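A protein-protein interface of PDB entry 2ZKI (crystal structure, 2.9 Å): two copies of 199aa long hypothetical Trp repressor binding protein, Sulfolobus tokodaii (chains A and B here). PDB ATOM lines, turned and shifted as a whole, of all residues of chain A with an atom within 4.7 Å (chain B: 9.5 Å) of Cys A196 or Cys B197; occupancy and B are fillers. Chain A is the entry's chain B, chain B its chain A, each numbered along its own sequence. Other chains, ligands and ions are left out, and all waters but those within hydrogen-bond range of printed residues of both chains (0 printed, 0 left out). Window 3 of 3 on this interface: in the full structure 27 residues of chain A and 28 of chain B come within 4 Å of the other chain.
The backbone carbonyl oxygen (O) of Ala A193 is in hydrogen-bond range of the side-chain sulfur (SG) of Cys B197, 3.6 Å away. The side-chain sulfur of Cys B197 sits close to the backbone carbonyl oxygen of Cys A196, 3.5 Å away. SG of Cys B197 sits at hydrogen-bond distance from N of Cys A197, at 3.5 Å.
OD1 of Asn B198 lies close to SG of Cys B197 (3.7 Å). The side-chain amino group (NZ) of Lys A192 sits at hydrogen-bond distance from the backbone carbonyl oxygen (O) of Cys A3 (2.8 Å). SG of Cys A3 is disulfide-bonded to SG of Cys A196, at 2.0 Å. The side-chain sulfur (SG) of Cys B3 is disulfide-bonded to the side-chain sulfur (SG) of Cys B196.
Lys A192 touches Asn B198 (CE to ND2, 3.6 Å). Ala A193 touches Ala B193 (CB to O, 3.4 Å). OD1 of Asn B198 touches CA of Ala A193 (3.96 Å). Cys A197 touches Lys B192 (SG to CD, 3.997 Å). SG of Cys A197 touches CA of Ala B193, at 3.9 Å.
Of chain B, only Cys B197 (3.4 Å) comes within 4 Å of Cys A196. Of the printed residues of chain A, Cys B197 touches Ala A193 (3.6 Å), Cys A196 (3.4 Å) and Cys A197 (3.5 Å). No residue of chain B comes within 4 Å of Cys A3. Ala A193 touches just these residues of chain B: Ala B193, Cys B197 and Asn B198. Of the printed residues of chain A, Lys B192 touches Cys A197 (3.997 Å). Printed residues of chain A within 4 Å of Asn B198: Lys A192 (3.6 Å) and Ala A193 (3.96 Å). Printed residues of chain A within 4 Å of Ala B193: Ala A193 (3.4 Å) and Cys A197 (3.9 Å). Glu B189 touches none of the printed residues of chain A. The nearest residue of chain B that does not touch Cys A196 is Asn B198 (5.5 Å). The nearest residue of chain A that does not touch Cys B197 is Lys A192 (4.4 Å).
Printed residues of chain B that touch a printed residue of chain A: Lys B192, Ala B193, Cys B197 and Asn B198. Hydrophobic or aromatic side chains of chain B within 4 Å of the printed part of chain A: Ala B193. Hydrophobic or aromatic side chains of chain A within 4 Å of the printed part of chain B: Ala A193. Among the printed residues, 8 pairs touch across the chains. Among the printed residues, no Asp or Glu carboxylate lies within 4 Å of a Lys or Arg side-chain nitrogen of the other chain.
Ala B193 touches its own counterpart, Ala A193. Ala A193 touches Cys B197, and with the chains exchanged Cys A197 touches Ala B193. Cys A196 touches Cys B197, but with the chains exchanged Cys A197 does not touch Cys B196 (6.2 Å). Cys B197 touches its own counterpart, Cys A197. Of the 8 pairs that touch across the chains among the printed residues, 4 have their exchanged pair printed and touching as well.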
ATOM      1  N   CYS A   3      21.854 -26.471  -5.063  1.00  0.00           N
ATOM      2  CA  CYS A   3      20.488 -25.870  -5.053  1.00  0.00           C
ATOM      3  C   CYS A   3      19.568 -26.537  -6.080  1.00  0.00           C
ATOM      4  O   CYS A   3      19.622 -26.225  -7.275  1.00  0.00           O
ATOM      5  CB  CYS A   3      20.561 -24.356  -5.307  1.00  0.00           C
ATOM      6  SG  CYS A   3      18.996 -23.461  -5.023  1.00  0.00           S
ATOM      7  N   LYS A 192      13.415 -23.401  -9.828  1.00  0.00           N
ATOM      8  CA  LYS A 192      14.834 -23.243  -9.513  1.00  0.00           C
ATOM      9  C   LYS A 192      15.246 -21.769  -9.547  1.00  0.00           C
ATOM     10  O   LYS A 192      16.031 -21.320  -8.712  1.00  0.00           O
ATOM     11  CB  LYS A 192      15.685 -24.064 -10.489  1.00  0.00           C
ATOM     12  CG  LYS A 192      17.169 -24.127 -10.155  1.00  0.00           C
ATOM     13  CD  LYS A 192      17.958 -24.799 -11.275  1.00  0.00           C
ATOM     14  CE  LYS A 192      19.463 -24.613 -11.098  1.00  0.00           C
ATOM     15  NZ  LYS A 192      20.008 -25.372  -9.934  1.00  0.00           N
ATOM     16  N   ALA A 193      14.704 -21.028 -10.512  1.00  0.00           N
ATOM     17  CA  ALA A 193      14.983 -19.600 -10.657  1.00  0.00           C
ATOM     18  C   ALA A 193      14.506 -18.784  -9.453  1.00  0.00           C
ATOM     19  O   ALA A 193      15.202 -17.867  -9.009  1.00  0.00           O
ATOM     20  CB  ALA A 193      14.369 -19.066 -11.941  1.00  0.00           C
ATOM     21  N   ILE A 194      13.328 -19.124  -8.927  1.00  0.00           N
ATOM     22  CA  ILE A 194      12.751 -18.414  -7.778  1.00  0.00           C
ATOM     23  C   ILE A 194      13.433 -18.804  -6.460  1.00  0.00           C
ATOM     24  O   ILE A 194      13.687 -17.945  -5.613  1.00  0.00           O
ATOM     25  CB  ILE A 194      11.208 -18.624  -7.668  1.00  0.00           C
ATOM     26  CG1 ILE A 194      10.509 -18.408  -9.022  1.00  0.00           C
ATOM     27  CG2 ILE A 194      10.601 -17.729  -6.578  1.00  0.00           C
ATOM     28  CD1 ILE A 194      10.622 -16.999  -9.605  1.00  0.00           C
ATOM     29  N   LYS A 195      13.734 -20.092  -6.304  1.00  0.00           N
ATOM     30  CA  LYS A 195      14.345 -20.618  -5.083  1.00  0.00           C
ATOM     31  C   LYS A 195      15.809 -20.197  -4.913  1.00  0.00           C
ATOM     32  O   LYS A 195      16.184 -19.665  -3.869  1.00  0.00           O
ATOM     33  CB  LYS A 195      14.223 -22.146  -5.038  1.00  0.00           C
ATOM     34  CG  LYS A 195      14.663 -22.777  -3.725  1.00  0.00           C
ATOM     35  CD  LYS A 195      14.765 -24.293  -3.843  1.00  0.00           C
ATOM     36  CE  LYS A 195      15.258 -24.931  -2.545  1.00  0.00           C
ATOM     37  NZ  LYS A 195      14.249 -24.848  -1.445  1.00  0.00           N
ATOM     38  N   CYS A 196      16.623 -20.430  -5.943  1.00  0.00           N
ATOM     39  CA  CYS A 196      18.075 -20.228  -5.863  1.00  0.00           C
ATOM     40  C   CYS A 196      18.521 -18.763  -5.978  1.00  0.00           C
ATOM     41  O   CYS A 196      19.721 -18.476  -5.987  1.00  0.00           O
ATOM     42  CB  CYS A 196      18.787 -21.085  -6.921  1.00  0.00           C
ATOM     43  SG  CYS A 196      18.388 -22.865  -6.875  1.00  0.00           S
ATOM     44  N   CYS A 197      17.557 -17.846  -6.057  1.00  0.00           N
ATOM     45  CA  CYS A 197      17.833 -16.415  -6.235  1.00  0.00           C
ATOM     46  C   CYS A 197      18.262 -15.742  -4.932  1.00  0.00           C
ATOM     47  O   CYS A 197      17.565 -15.823  -3.917  1.00  0.00           O
ATOM     48  CB  CYS A 197      16.606 -15.708  -6.827  1.00  0.00           C
ATOM     49  SG  CYS A 197      16.905 -14.027  -7.443  1.00  0.00           S
ATOM     50  N   CYS B   3      23.660  -7.051 -12.612  1.00  0.00           N
ATOM     51  CA  CYS B   3      22.435  -7.510 -13.330  1.00  0.00           C
ATOM     52  C   CYS B   3      21.208  -6.709 -12.894  1.00  0.00           C
ATOM     53  O   CYS B   3      20.908  -6.612 -11.701  1.00  0.00           O
ATOM     54  CB  CYS B   3      22.206  -9.009 -13.102  1.00  0.00           C
ATOM     55  SG  CYS B   3      20.935  -9.748 -14.172  1.00  0.00           S
ATOM     56  N   LYS B   4      20.506  -6.141 -13.874  1.00  0.00           N
ATOM     57  CA  LYS B   4      19.358  -5.273 -13.621  1.00  0.00           C
ATOM     58  C   LYS B   4      18.272  -5.526 -14.674  1.00  0.00           C
ATOM     59  O   LYS B   4      18.555  -5.485 -15.873  1.00  0.00           O
ATOM     60  CB  LYS B   4      19.802  -3.808 -13.652  1.00  0.00           C
ATOM     61  CG  LYS B   4      18.904  -2.847 -12.896  1.00  0.00           C
ATOM     62  CD  LYS B   4      19.356  -1.411 -13.118  1.00  0.00           C
ATOM     63  CE  LYS B   4      18.605  -0.436 -12.222  1.00  0.00           C
ATOM     64  NZ  LYS B   4      19.052   0.967 -12.451  1.00  0.00           N
ATOM     65  N   GLU B 189      10.835  -8.419  -9.137  1.00  0.00           N
ATOM     66  CA  GLU B 189      11.420  -9.541  -8.401  1.00  0.00           C
ATOM     67  C   GLU B 189      11.485 -10.818  -9.233  1.00  0.00           C
ATOM     68  O   GLU B 189      12.482 -11.539  -9.199  1.00  0.00           O
ATOM     69  CB  GLU B 189      10.651  -9.797  -7.101  1.00  0.00           C
ATOM     70  CG  GLU B 189      10.934  -8.778  -6.006  1.00  0.00           C
ATOM     71  CD  GLU B 189      10.275  -9.126  -4.684  1.00  0.00           C
ATOM     72  OE1 GLU B 189       9.047  -9.367  -4.664  1.00  0.00           O
ATOM     73  OE2 GLU B 189      10.989  -9.151  -3.657  1.00  0.00           O
ATOM     74  N   VAL B 190      10.420 -11.086  -9.982  1.00  0.00           N
ATOM     75  CA  VAL B 190      10.351 -12.265 -10.840  1.00  0.00           C
ATOM     76  C   VAL B 190      11.238 -12.075 -12.073  1.00  0.00           C
ATOM     77  O   VAL B 190      11.854 -13.028 -12.559  1.00  0.00           O
ATOM     78  CB  VAL B 190       8.892 -12.574 -11.262  1.00  0.00           C
ATOM     79  CG1 VAL B 190       8.800 -13.932 -11.955  1.00  0.00           C
ATOM     80  CG2 VAL B 190       7.971 -12.541 -10.050  1.00  0.00           C
ATOM     81  N   ALA B 191      11.308 -10.837 -12.557  1.00  0.00           N
ATOM     82  CA  ALA B 191      12.093 -10.499 -13.740  1.00  0.00           C
ATOM     83  C   ALA B 191      13.585 -10.759 -13.553  1.00  0.00           C
ATOM     84  O   ALA B 191      14.236 -11.315 -14.442  1.00  0.00           O
ATOM     85  CB  ALA B 191      11.850  -9.055 -14.142  1.00  0.00           C
ATOM     86  N   LYS B 192      14.118 -10.364 -12.398  1.00  0.00           N
ATOM     87  CA  LYS B 192      15.536 -10.571 -12.103  1.00  0.00           C
ATOM     88  C   LYS B 192      15.849 -12.006 -11.680  1.00  0.00           C
ATOM     89  O   LYS B 192      16.994 -12.443 -11.767  1.00  0.00           O
ATOM     90  CB  LYS B 192      16.068  -9.539 -11.090  1.00  0.00           C
ATOM     91  CG  LYS B 192      15.399  -9.533  -9.716  1.00  0.00           C
ATOM     92  CD  LYS B 192      16.213 -10.286  -8.667  1.00  0.00           C
ATOM     93  CE  LYS B 192      17.417  -9.477  -8.184  1.00  0.00           C
ATOM     94  NZ  LYS B 192      18.086 -10.125  -7.017  1.00  0.00           N
ATOM     95  N   ALA B 193      14.830 -12.738 -11.238  1.00  0.00           N
ATOM     96  CA  ALA B 193      14.992 -14.143 -10.874  1.00  0.00           C
ATOM     97  C   ALA B 193      15.167 -15.031 -12.108  1.00  0.00           C
ATOM     98  O   ALA B 193      15.930 -15.997 -12.081  1.00  0.00           O
ATOM     99  CB  ALA B 193      13.815 -14.619 -10.033  1.00  0.00           C
ATOM    100  N   ILE B 194      14.460 -14.694 -13.185  1.00  0.00           N
ATOM    101  CA  ILE B 194      14.549 -15.438 -14.443  1.00  0.00           C
ATOM    102  C   ILE B 194      15.823 -15.073 -15.204  1.00  0.00           C
ATOM    103  O   ILE B 194      16.520 -15.953 -15.713  1.00  0.00           O
ATOM    104  CB  ILE B 194      13.290 -15.212 -15.337  1.00  0.00           C
ATOM    105  CG1 ILE B 194      12.016 -15.717 -14.639  1.00  0.00           C
ATOM    106  CG2 ILE B 194      13.458 -15.858 -16.723  1.00  0.00           C
ATOM    107  CD1 ILE B 194      11.881 -17.240 -14.531  1.00  0.00           C
ATOM    108  N   LYS B 195      16.125 -13.778 -15.263  1.00  0.00           N
ATOM    109  CA  LYS B 195      17.269 -13.273 -16.018  1.00  0.00           C
ATOM    110  C   LYS B 195      18.614 -13.563 -15.339  1.00  0.00           C
ATOM    111  O   LYS B 195      19.476 -14.227 -15.920  1.00  0.00           O
ATOM    112  CB  LYS B 195      17.113 -11.769 -16.266  1.00  0.00           C
ATOM    113  CG  LYS B 195      18.174 -11.155 -17.163  1.00  0.00           C
ATOM    114  CD  LYS B 195      18.091  -9.639 -17.132  1.00  0.00           C
ATOM    115  CE  LYS B 195      19.028  -9.006 -18.148  1.00  0.00           C
ATOM    116  NZ  LYS B 195      18.948  -7.517 -18.124  1.00  0.00           N
ATOM    117  N   CYS B 196      18.775 -13.075 -14.110  1.00  0.00           N
ATOM    118  CA  CYS B 196      20.072 -13.075 -13.425  1.00  0.00           C
ATOM    119  C   CYS B 196      20.468 -14.422 -12.826  1.00  0.00           C
ATOM    120  O   CYS B 196      21.594 -14.881 -13.022  1.00  0.00           O
ATOM    121  CB  CYS B 196      20.100 -12.002 -12.335  1.00  0.00           C
ATOM    122  SG  CYS B 196      19.504 -10.387 -12.874  1.00  0.00           S
ATOM    123  N   CYS B 197      19.541 -15.042 -12.098  1.00  0.00           N
ATOM    124  CA  CYS B 197      19.809 -16.272 -11.347  1.00  0.00           C
ATOM    125  C   CYS B 197      20.434 -17.397 -12.190  1.00  0.00           C
ATOM    126  O   CYS B 197      21.355 -18.081 -11.732  1.00  0.00           O
ATOM    127  CB  CYS B 197      18.532 -16.758 -10.662  1.00  0.00           C
ATOM    128  SG  CYS B 197      18.794 -17.909  -9.303  1.00  0.00           S
ATOM    129  N   ASN B 198      19.937 -17.576 -13.415  1.00  0.00           N
ATOM    130  CA  ASN B 198      20.489 -18.568 -14.344  1.00  0.00           C
ATOM    131  C   ASN B 198      20.778 -17.978 -15.721  1.00  0.00           C
ATOM    132  O   ASN B 198      21.777 -18.318 -16.356  1.00  0.00           O
ATOM    133  CB  ASN B 198      19.559 -19.781 -14.476  1.00  0.00           C
ATOM    134  CG  ASN B 198      19.340 -20.498 -13.154  1.00  0.00           C
ATOM    135  OD1 ASN B 198      18.553 -20.050 -12.316  1.00  0.00           O
ATOM    136  ND2 ASN B 198      20.029 -21.623 -12.967  1.00  0.00           N
